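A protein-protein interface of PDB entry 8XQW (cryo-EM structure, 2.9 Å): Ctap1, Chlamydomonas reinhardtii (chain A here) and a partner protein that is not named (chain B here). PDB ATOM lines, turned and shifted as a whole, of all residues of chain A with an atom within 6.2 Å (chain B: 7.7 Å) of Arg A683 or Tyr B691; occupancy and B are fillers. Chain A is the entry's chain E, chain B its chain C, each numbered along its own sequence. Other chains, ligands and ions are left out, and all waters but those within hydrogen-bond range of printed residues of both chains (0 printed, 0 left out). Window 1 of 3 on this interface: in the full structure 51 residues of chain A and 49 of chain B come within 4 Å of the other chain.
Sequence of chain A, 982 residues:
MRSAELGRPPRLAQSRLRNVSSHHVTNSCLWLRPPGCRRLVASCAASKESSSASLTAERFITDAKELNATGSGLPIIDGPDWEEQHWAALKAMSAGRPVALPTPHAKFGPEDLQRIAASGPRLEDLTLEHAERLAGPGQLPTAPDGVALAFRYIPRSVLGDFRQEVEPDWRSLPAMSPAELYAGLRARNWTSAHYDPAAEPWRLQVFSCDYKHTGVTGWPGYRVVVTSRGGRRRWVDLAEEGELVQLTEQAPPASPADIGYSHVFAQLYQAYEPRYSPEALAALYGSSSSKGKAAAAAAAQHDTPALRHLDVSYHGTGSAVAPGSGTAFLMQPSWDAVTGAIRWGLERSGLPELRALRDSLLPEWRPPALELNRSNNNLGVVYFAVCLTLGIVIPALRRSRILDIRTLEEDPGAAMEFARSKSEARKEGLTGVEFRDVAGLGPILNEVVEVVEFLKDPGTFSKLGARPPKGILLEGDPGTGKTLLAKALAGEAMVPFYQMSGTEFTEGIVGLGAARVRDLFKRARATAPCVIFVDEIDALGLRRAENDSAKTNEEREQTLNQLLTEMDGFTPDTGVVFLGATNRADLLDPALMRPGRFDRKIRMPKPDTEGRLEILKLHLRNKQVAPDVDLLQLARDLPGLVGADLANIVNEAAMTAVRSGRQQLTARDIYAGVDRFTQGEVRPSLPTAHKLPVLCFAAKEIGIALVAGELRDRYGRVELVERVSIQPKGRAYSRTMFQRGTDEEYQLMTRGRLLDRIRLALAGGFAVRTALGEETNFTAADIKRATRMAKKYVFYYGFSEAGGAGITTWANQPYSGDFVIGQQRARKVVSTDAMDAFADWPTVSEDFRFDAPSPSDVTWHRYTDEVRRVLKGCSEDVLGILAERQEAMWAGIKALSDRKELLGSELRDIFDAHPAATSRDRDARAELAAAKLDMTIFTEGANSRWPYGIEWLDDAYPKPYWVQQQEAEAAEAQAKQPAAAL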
ATOM      1  N   GLU A 681       2.553  -3.994   5.307  1.00  0.00           N
ATOM      2  CA  GLU A 681       1.305  -4.527   5.827  1.00  0.00           C
ATOM      3  C   GLU A 681       0.787  -5.652   4.940  1.00  0.00           C
ATOM      4  O   GLU A 681       1.088  -5.731   3.750  1.00  0.00           O
ATOM      5  CB  GLU A 681       0.256  -3.424   5.927  1.00  0.00           C
ATOM      6  CG  GLU A 681      -0.245  -2.929   4.581  1.00  0.00           C
ATOM      7  CD  GLU A 681       0.768  -2.067   3.855  1.00  0.00           C
ATOM      8  OE1 GLU A 681       1.812  -1.740   4.457  1.00  0.00           O
ATOM      9  OE2 GLU A 681       0.523  -1.723   2.681  1.00  0.00           O
ATOM     10  N   VAL A 682      -0.009  -6.534   5.541  1.00  0.00           N
ATOM     11  CA  VAL A 682      -0.573  -7.641   4.787  1.00  0.00           C
ATOM     12  C   VAL A 682      -1.620  -7.109   3.817  1.00  0.00           C
ATOM     13  O   VAL A 682      -2.147  -6.003   3.979  1.00  0.00           O
ATOM     14  CB  VAL A 682      -1.176  -8.696   5.732  1.00  0.00           C
ATOM     15  CG1 VAL A 682      -1.207 -10.056   5.058  1.00  0.00           C
ATOM     16  CG2 VAL A 682      -0.385  -8.757   7.014  1.00  0.00           C
ATOM     17  N   ARG A 683      -1.915  -7.894   2.795  1.00  0.00           N
ATOM     18  CA  ARG A 683      -2.865  -7.523   1.762  1.00  0.00           C
ATOM     19  C   ARG A 683      -3.721  -8.734   1.436  1.00  0.00           C
ATOM     20  O   ARG A 683      -3.346  -9.867   1.755  1.00  0.00           O
ATOM     21  CB  ARG A 683      -2.141  -7.012   0.511  1.00  0.00           C
ATOM     22  CG  ARG A 683      -1.308  -5.781   0.770  1.00  0.00           C
ATOM     23  CD  ARG A 683      -0.930  -5.084  -0.513  1.00  0.00           C
ATOM     24  NE  ARG A 683      -0.399  -3.754  -0.248  1.00  0.00           N
ATOM     25  CZ  ARG A 683      -0.146  -2.851  -1.185  1.00  0.00           C
ATOM     26  NH1 ARG A 683      -0.372  -3.133  -2.458  1.00  0.00           N
ATOM     27  NH2 ARG A 683       0.336  -1.664  -0.849  1.00  0.00           N
ATOM     28  N   PRO A 684      -4.887  -8.529   0.823  1.00  0.00           N
ATOM     29  CA  PRO A 684      -5.791  -9.654   0.576  1.00  0.00           C
ATOM     30  C   PRO A 684      -5.146 -10.735  -0.273  1.00  0.00           C
ATOM     31  O   PRO A 684      -4.308 -10.468  -1.132  1.00  0.00           O
ATOM     32  CB  PRO A 684      -6.973  -9.005  -0.154  1.00  0.00           C
ATOM     33  CG  PRO A 684      -6.475  -7.684  -0.610  1.00  0.00           C
ATOM     34  CD  PRO A 684      -5.502  -7.256   0.424  1.00  0.00           C
ATOM     35  N   SER A 685      -5.569 -11.967  -0.026  1.00  0.00           N
ATOM     36  CA  SER A 685      -4.969 -13.132  -0.646  1.00  0.00           C
ATOM     37  C   SER A 685      -5.201 -13.148  -2.152  1.00  0.00           C
ATOM     38  O   SER A 685      -5.974 -12.360  -2.700  1.00  0.00           O
ATOM     39  CB  SER A 685      -5.541 -14.402  -0.027  1.00  0.00           C
ATOM     40  OG  SER A 685      -6.606 -14.897  -0.818  1.00  0.00           O
ATOM     41  N   GLN A 727       1.781 -15.254   0.199  1.00  0.00           N
ATOM     42  CA  GLN A 727       0.829 -14.329   0.785  1.00  0.00           C
ATOM     43  C   GLN A 727       1.157 -12.921   0.319  1.00  0.00           C
ATOM     44  O   GLN A 727       2.202 -12.385   0.707  1.00  0.00           O
ATOM     45  CB  GLN A 727       0.882 -14.399   2.299  1.00  0.00           C
ATOM     46  CG  GLN A 727      -0.471 -14.497   2.970  1.00  0.00           C
ATOM     47  CD  GLN A 727      -1.420 -13.396   2.553  1.00  0.00           C
ATOM     48  OE1 GLN A 727      -1.036 -12.235   2.446  1.00  0.00           O
ATOM     49  NE2 GLN A 727      -2.672 -13.759   2.313  1.00  0.00           N
ATOM     50  N   PRO A 728       0.331 -12.298  -0.518  1.00  0.00           N
ATOM     51  CA  PRO A 728       0.620 -10.930  -0.954  1.00  0.00           C
ATOM     52  C   PRO A 728       0.803 -10.007   0.235  1.00  0.00           C
ATOM     53  O   PRO A 728      -0.100  -9.827   1.049  1.00  0.00           O
ATOM     54  CB  PRO A 728      -0.616 -10.556  -1.772  1.00  0.00           C
ATOM     55  CG  PRO A 728      -1.108 -11.834  -2.268  1.00  0.00           C
ATOM     56  CD  PRO A 728      -0.851 -12.841  -1.195  1.00  0.00           C
ATOM     57  N   LYS A 729       1.988  -9.415   0.324  1.00  0.00           N
ATOM     58  CA  LYS A 729       2.401  -8.711   1.532  1.00  0.00           C
ATOM     59  C   LYS A 729       3.374  -7.618   1.113  1.00  0.00           C
ATOM     60  O   LYS A 729       4.496  -7.912   0.700  1.00  0.00           O
ATOM     61  CB  LYS A 729       3.034  -9.681   2.514  1.00  0.00           C
ATOM     62  CG  LYS A 729       3.719  -9.050   3.695  1.00  0.00           C
ATOM     63  CD  LYS A 729       4.487 -10.103   4.467  1.00  0.00           C
ATOM     64  CE  LYS A 729       3.638 -11.340   4.683  1.00  0.00           C
ATOM     65  NZ  LYS A 729       4.340 -12.356   5.503  1.00  0.00           N
ATOM     66  N   GLY A 730       2.948  -6.390   1.212  1.00  0.00           N
ATOM     67  CA  GLY A 730       3.803  -5.273   0.817  1.00  0.00           C
ATOM     68  C   GLY A 730       3.560  -4.870  -0.636  1.00  0.00           C
ATOM     69  O   GLY A 730       2.499  -4.372  -0.961  1.00  0.00           O
ATOM     70  N   ARG A 731       4.557  -5.095  -1.486  1.00  0.00           N
ATOM     71  CA  ARG A 731       4.426  -4.840  -2.915  1.00  0.00           C
ATOM     72  C   ARG A 731       4.504  -6.103  -3.755  1.00  0.00           C
ATOM     73  O   ARG A 731       3.997  -6.120  -4.875  1.00  0.00           O
ATOM     74  CB  ARG A 731       5.498  -3.859  -3.383  1.00  0.00           C
ATOM     75  CG  ARG A 731       5.266  -2.437  -2.929  1.00  0.00           C
ATOM     76  CD  ARG A 731       6.039  -1.466  -3.794  1.00  0.00           C
ATOM     77  NE  ARG A 731       6.575  -0.352  -3.021  1.00  0.00           N
ATOM     78  CZ  ARG A 731       7.735  -0.384  -2.374  1.00  0.00           C
ATOM     79  NH1 ARG A 731       8.484  -1.479  -2.402  1.00  0.00           N
ATOM     80  NH2 ARG A 731       8.149   0.676  -1.695  1.00  0.00           N
ATOM     81  N   ASN B 530     -16.181  -3.354   2.401  1.00  0.00           N
ATOM     82  CA  ASN B 530     -15.994  -4.630   1.733  1.00  0.00           C
ATOM     83  C   ASN B 530     -14.553  -5.101   1.868  1.00  0.00           C
ATOM     84  O   ASN B 530     -13.636  -4.317   2.122  1.00  0.00           O
ATOM     85  CB  ASN B 530     -16.360  -4.520   0.250  1.00  0.00           C
ATOM     86  CG  ASN B 530     -15.615  -3.394  -0.447  1.00  0.00           C
ATOM     87  OD1 ASN B 530     -15.347  -2.348   0.148  1.00  0.00           O
ATOM     88  ND2 ASN B 530     -15.269  -3.609  -1.708  1.00  0.00           N
ATOM     89  N   GLY B 531     -14.371  -6.408   1.693  1.00  0.00           N
ATOM     90  CA  GLY B 531     -13.047  -6.993   1.544  1.00  0.00           C
ATOM     91  C   GLY B 531     -12.078  -6.690   2.663  1.00  0.00           C
ATOM     92  O   GLY B 531     -10.863  -6.724   2.446  1.00  0.00           O
ATOM     93  N   ILE B 532     -12.581  -6.398   3.859  1.00  0.00           N
ATOM     94  CA  ILE B 532     -11.717  -6.003   4.964  1.00  0.00           C
ATOM     95  C   ILE B 532     -11.831  -7.020   6.089  1.00  0.00           C
ATOM     96  O   ILE B 532     -11.731  -6.668   7.267  1.00  0.00           O
ATOM     97  CB  ILE B 532     -12.044  -4.583   5.459  1.00  0.00           C
ATOM     98  CG1 ILE B 532     -13.509  -4.443   5.864  1.00  0.00           C
ATOM     99  CG2 ILE B 532     -11.660  -3.551   4.413  1.00  0.00           C
ATOM    100  CD1 ILE B 532     -13.731  -3.315   6.836  1.00  0.00           C
ATOM    101  N   GLU B 534      -9.809  -9.409   7.158  1.00  0.00           N
ATOM    102  CA  GLU B 534      -8.633  -9.420   8.023  1.00  0.00           C
ATOM    103  C   GLU B 534      -8.654  -8.242   8.985  1.00  0.00           C
ATOM    104  O   GLU B 534      -8.596  -8.424  10.208  1.00  0.00           O
ATOM    105  CB  GLU B 534      -7.363  -9.391   7.175  1.00  0.00           C
ATOM    106  CG  GLU B 534      -6.883 -10.754   6.721  1.00  0.00           C
ATOM    107  CD  GLU B 534      -6.048 -10.676   5.457  1.00  0.00           C
ATOM    108  OE1 GLU B 534      -6.325 -11.437   4.505  1.00  0.00           O
ATOM    109  OE2 GLU B 534      -5.115  -9.847   5.413  1.00  0.00           O
ATOM    110  N   VAL B 535      -8.785  -7.026   8.457  1.00  0.00           N
ATOM    111  CA  VAL B 535      -8.747  -5.872   9.339  1.00  0.00           C
ATOM    112  C   VAL B 535     -10.059  -5.721  10.099  1.00  0.00           C
ATOM    113  O   VAL B 535     -10.111  -5.000  11.093  1.00  0.00           O
ATOM    114  CB  VAL B 535      -8.369  -4.593   8.563  1.00  0.00           C
ATOM    115  CG1 VAL B 535      -6.953  -4.708   8.010  1.00  0.00           C
ATOM    116  CG2 VAL B 535      -9.349  -4.319   7.461  1.00  0.00           C
ATOM    117  N   LEU B 564      -2.683   4.155  11.737  1.00  0.00           N
ATOM    118  CA  LEU B 564      -2.604   4.753  10.414  1.00  0.00           C
ATOM    119  C   LEU B 564      -3.528   4.017   9.457  1.00  0.00           C
ATOM    120  O   LEU B 564      -3.647   2.790   9.508  1.00  0.00           O
ATOM    121  CB  LEU B 564      -1.176   4.716   9.867  1.00  0.00           C
ATOM    122  CG  LEU B 564      -0.108   5.546  10.567  1.00  0.00           C
ATOM    123  CD1 LEU B 564       1.174   5.470   9.774  1.00  0.00           C
ATOM    124  CD2 LEU B 564      -0.551   6.982  10.725  1.00  0.00           C
ATOM    125  N   LEU B 565      -4.185   4.782   8.590  1.00  0.00           N
ATOM    126  CA  LEU B 565      -5.045   4.255   7.534  1.00  0.00           C
ATOM    127  C   LEU B 565      -4.306   4.408   6.212  1.00  0.00           C
ATOM    128  O   LEU B 565      -4.168   5.523   5.701  1.00  0.00           O
ATOM    129  CB  LEU B 565      -6.385   4.987   7.482  1.00  0.00           C
ATOM    130  CG  LEU B 565      -7.161   5.307   8.756  1.00  0.00           C
ATOM    131  CD1 LEU B 565      -8.197   6.364   8.458  1.00  0.00           C
ATOM    132  CD2 LEU B 565      -7.834   4.080   9.299  1.00  0.00           C
ATOM    133  N   ALA B 566      -3.892   3.277   5.650  1.00  0.00           N
ATOM    134  CA  ALA B 566      -3.194   3.310   4.353  1.00  0.00           C
ATOM    135  C   ALA B 566      -4.114   2.738   3.282  1.00  0.00           C
ATOM    136  O   ALA B 566      -4.854   1.780   3.573  1.00  0.00           O
ATOM    137  CB  ALA B 566      -1.919   2.524   4.434  1.00  0.00           C
ATOM    138  N   GLY B 567      -4.076   3.317   2.085  1.00  0.00           N
ATOM    139  CA  GLY B 567      -4.869   2.786   0.969  1.00  0.00           C
ATOM    140  C   GLY B 567      -4.307   3.338  -0.314  1.00  0.00           C
ATOM    141  O   GLY B 567      -3.119   3.090  -0.583  1.00  0.00           O
ATOM    142  N   ALA B 568      -5.113   4.097  -1.054  1.00  0.00           N
ATOM    143  CA  ALA B 568      -4.669   4.666  -2.344  1.00  0.00           C
ATOM    144  C   ALA B 568      -5.541   5.868  -2.695  1.00  0.00           C
ATOM    145  O   ALA B 568      -6.702   5.931  -2.253  1.00  0.00           O
ATOM    146  CB  ALA B 568      -4.758   3.602  -3.404  1.00  0.00           C
ATOM    147  N   THR B 571      -9.536   6.145  -1.840  1.00  0.00           N
ATOM    148  CA  THR B 571     -10.002   5.055  -0.959  1.00  0.00           C
ATOM    149  C   THR B 571     -11.060   5.595  -0.020  1.00  0.00           C
ATOM    150  O   THR B 571     -11.868   4.787   0.476  1.00  0.00           O
ATOM    151  CB  THR B 571      -8.806   4.436  -0.241  1.00  0.00           C
ATOM    152  OG1 THR B 571      -7.940   4.001  -1.283  1.00  0.00           O
ATOM    153  CG2 THR B 571      -9.173   3.228   0.598  1.00  0.00           C
ATOM    154  N   LYS B 573     -11.086   6.936   3.108  1.00  0.00           N
ATOM    155  CA  LYS B 573     -10.959   6.190   4.354  1.00  0.00           C
ATOM    156  C   LYS B 573     -11.802   6.790   5.468  1.00  0.00           C
ATOM    157  O   LYS B 573     -12.182   6.068   6.397  1.00  0.00           O
ATOM    158  CB  LYS B 573      -9.494   6.130   4.767  1.00  0.00           C
ATOM    159  CG  LYS B 573      -8.586   5.580   3.688  1.00  0.00           C
ATOM    160  CD  LYS B 573      -7.494   6.569   3.337  1.00  0.00           C
ATOM    161  CE  LYS B 573      -6.524   5.971   2.333  1.00  0.00           C
ATOM    162  NZ  LYS B 573      -5.478   6.943   1.924  1.00  0.00           N
ATOM    163  N   LEU B 576     -14.692   4.579   6.677  1.00  0.00           N
ATOM    164  CA  LEU B 576     -14.407   3.577   7.702  1.00  0.00           C
ATOM    165  C   LEU B 576     -14.376   4.202   9.086  1.00  0.00           C
ATOM    166  O   LEU B 576     -15.031   3.709  10.012  1.00  0.00           O
ATOM    167  CB  LEU B 576     -13.081   2.882   7.408  1.00  0.00           C
ATOM    168  CG  LEU B 576     -12.478   2.085   8.569  1.00  0.00           C
ATOM    169  CD1 LEU B 576     -13.378   0.930   8.984  1.00  0.00           C
ATOM    170  CD2 LEU B 576     -11.091   1.585   8.213  1.00  0.00           C
ATOM    171  N   THR B 670      -2.950   8.138   5.321  1.00  0.00           N
ATOM    172  CA  THR B 670      -2.096   8.539   4.214  1.00  0.00           C
ATOM    173  C   THR B 670      -1.832   7.353   3.306  1.00  0.00           C
ATOM    174  O   THR B 670      -2.024   6.195   3.678  1.00  0.00           O
ATOM    175  CB  THR B 670      -0.766   9.111   4.687  1.00  0.00           C
ATOM    176  OG1 THR B 670      -0.009   9.523   3.544  1.00  0.00           O
ATOM    177  CG2 THR B 670       0.012   8.051   5.441  1.00  0.00           C
ATOM    178  N   ASN B 671      -1.355   7.664   2.103  1.00  0.00           N
ATOM    179  CA  ASN B 671      -1.148   6.663   1.068  1.00  0.00           C
ATOM    180  C   ASN B 671       0.238   6.044   1.106  1.00  0.00           C
ATOM    181  O   ASN B 671       0.402   4.893   0.692  1.00  0.00           O
ATOM    182  CB  ASN B 671      -1.371   7.285  -0.306  1.00  0.00           C
ATOM    183  CG  ASN B 671      -0.385   8.389  -0.598  1.00  0.00           C
ATOM    184  OD1 ASN B 671       0.009   9.134   0.300  1.00  0.00           O
ATOM    185  ND2 ASN B 671       0.040   8.492  -1.851  1.00  0.00           N
ATOM    186  N   PRO B 673       2.871   4.775   3.507  1.00  0.00           N
ATOM    187  CA  PRO B 673       3.301   4.453   4.875  1.00  0.00           C
ATOM    188  C   PRO B 673       4.804   4.367   5.037  1.00  0.00           C
ATOM    189  O   PRO B 673       5.292   4.513   6.164  1.00  0.00           O
ATOM    190  CB  PRO B 673       2.643   3.093   5.136  1.00  0.00           C
ATOM    191  CG  PRO B 673       2.514   2.488   3.792  1.00  0.00           C
ATOM    192  CD  PRO B 673       2.259   3.618   2.835  1.00  0.00           C
ATOM    193  N   ILE B 689      -1.117  -0.225  11.628  1.00  0.00           N
ATOM    194  CA  ILE B 689      -1.458   0.285  10.310  1.00  0.00           C
ATOM    195  C   ILE B 689      -2.485  -0.646   9.687  1.00  0.00           C
ATOM    196  O   ILE B 689      -2.349  -1.873   9.754  1.00  0.00           O
ATOM    197  CB  ILE B 689      -0.211   0.431   9.418  1.00  0.00           C
ATOM    198  CG1 ILE B 689      -0.609   0.798   7.993  1.00  0.00           C
ATOM    199  CG2 ILE B 689       0.619  -0.833   9.448  1.00  0.00           C
ATOM    200  CD1 ILE B 689       0.552   0.855   7.047  1.00  0.00           C
ATOM    201  N   ILE B 690      -3.519  -0.057   9.096  1.00  0.00           N
ATOM    202  CA  ILE B 690      -4.634  -0.781   8.503  1.00  0.00           C
ATOM    203  C   ILE B 690      -4.719  -0.424   7.028  1.00  0.00           C
ATOM    204  O   ILE B 690      -4.744   0.755   6.662  1.00  0.00           O
ATOM    205  CB  ILE B 690      -5.955  -0.456   9.229  1.00  0.00           C
ATOM    206  CG1 ILE B 690      -7.134  -1.133   8.542  1.00  0.00           C
ATOM    207  CG2 ILE B 690      -6.165   1.032   9.346  1.00  0.00           C
ATOM    208  CD1 ILE B 690      -8.356  -1.208   9.407  1.00  0.00           C
ATOM    209  N   TYR B 691      -4.777  -1.447   6.182  1.00  0.00           N
ATOM    210  CA  TYR B 691      -4.773  -1.277   4.738  1.00  0.00           C
ATOM    211  C   TYR B 691      -6.186  -1.434   4.200  1.00  0.00           C
ATOM    212  O   TYR B 691      -6.817  -2.476   4.402  1.00  0.00           O
ATOM    213  CB  TYR B 691      -3.844  -2.293   4.075  1.00  0.00           C
ATOM    214  CG  TYR B 691      -3.776  -2.155   2.581  1.00  0.00           C
ATOM    215  CD1 TYR B 691      -3.193  -1.047   1.998  1.00  0.00           C
ATOM    216  CD2 TYR B 691      -4.292  -3.135   1.754  1.00  0.00           C
ATOM    217  CE1 TYR B 691      -3.127  -0.913   0.636  1.00  0.00           C
ATOM    218  CE2 TYR B 691      -4.232  -3.013   0.388  1.00  0.00           C
ATOM    219  CZ  TYR B 691      -3.649  -1.899  -0.169  1.00  0.00           C
ATOM    220  OH  TYR B 691      -3.587  -1.774  -1.537  1.00  0.00           O
ATOM    221  N   MET B 692      -6.674  -0.405   3.516  1.00  0.00           N
ATOM    222  CA  MET B 692      -8.008  -0.421   2.931  1.00  0.00           C
ATOM    223  C   MET B 692      -7.881  -0.629   1.433  1.00  0.00           C
ATOM    224  O   MET B 692      -7.380   0.263   0.731  1.00  0.00           O
ATOM    225  CB  MET B 692      -8.739   0.885   3.231  1.00  0.00           C
ATOM    226  CG  MET B 692     -10.203   0.713   3.581  1.00  0.00           C
ATOM    227  SD  MET B 692     -10.967   2.279   4.043  1.00  0.00           S
ATOM    228  CE  MET B 692     -12.670   1.986   3.575  1.00  0.00           C
ATOM    229  N   PRO B 693      -8.306  -1.766   0.897  1.00  0.00           N
ATOM    230  CA  PRO B 693      -8.027  -2.087  -0.501  1.00  0.00           C
ATOM    231  C   PRO B 693      -9.093  -1.568  -1.455  1.00  0.00           C
ATOM    232  O   PRO B 693     -10.155  -1.090  -1.054  1.00  0.00           O
ATOM    233  CB  PRO B 693      -8.022  -3.618  -0.487  1.00  0.00           C
ATOM    234  CG  PRO B 693      -9.054  -3.948   0.526  1.00  0.00           C
ATOM    235  CD  PRO B 693      -8.994  -2.872   1.580  1.00  0.00           C
ATOM    236  N   LEU B 694      -8.784  -1.685  -2.742  1.00  0.00           N
ATOM    237  CA  LEU B 694      -9.723  -1.293  -3.777  1.00  0.00           C
ATOM    238  C   LEU B 694     -10.878  -2.287  -3.850  1.00  0.00           C
ATOM    239  O   LEU B 694     -10.687  -3.490  -3.659  1.00  0.00           O
ATOM    240  CB  LEU B 694      -9.026  -1.216  -5.128  1.00  0.00           C
ATOM    241  CG  LEU B 694      -7.917  -0.177  -5.212  1.00  0.00           C
ATOM    242  CD1 LEU B 694      -7.343  -0.135  -6.609  1.00  0.00           C
ATOM    243  CD2 LEU B 694      -8.459   1.175  -4.811  1.00  0.00           C
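Among the printed residues, pairs that only touch across the chains: Arg A683 with Tyr B691, Glu A681 with Tyr B691, Glu A681 with Ile B689 and Val A682 with Glu B534.
Of chain B, only Tyr B691 comes within 4 Å of Arg A683.
Of chain A, only Glu A681 (3.7 Å) and Arg A683 (3.6 Å) come within 4 Å of Tyr B691.
Pro A684 touches none of the printed residues of chain B.
Of the printed residues of chain A, Glu B534 touches Val A682 (3.9 Å).
Printed residues of chain A within 4 Å of Ile B689: Glu A681.
Of the printed residues of chain B, Val A682 touches Glu B534.
Thr B571 touches none of the printed residues of chain A.
Ala B566 touches none of the printed residues of chain A.
The nearest residue of chain B that does not touch Arg A683 is Glu B534 (4.1 Å).
The nearest residue of chain A that does not touch Tyr B691 is Val A682 (4.1 Å).
OE2 of Glu A681 is in salt-bridge range of NH2 of Arg A683.
The backbone carbonyl oxygen of Glu A681 sits at hydrogen-bond distance from the backbone NH of Gly A730 (3.2 Å).
The side-chain amide oxygen (OE1) of Gln A727 lies close to the backbone carbonyl oxygen (O) of Arg A683 (3.4 Å).
The backbone carbonyl oxygen of Pro A728 is in hydrogen-bond range of the backbone NH of Arg A683, 3.2 Å away.
The guanidinium group (NE) of Arg A683 lies within hydrogen-bond range of the backbone carbonyl oxygen (O) of Gly A730.
Of the 22 printed residues of chain B, 3 touch a printed residue of chain A.
Hydrophobic or aromatic side chains of chain B that line the printed part of chain A: Ile B689 and Tyr B691.
Hydrophobic or aromatic side chains of chain A that line the printed part of chain B: Val A682.
Among the printed residues, no Asp or Glu carboxylate lies within 4 Å of a Lys or Arg side-chain nitrogen of the other chain.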
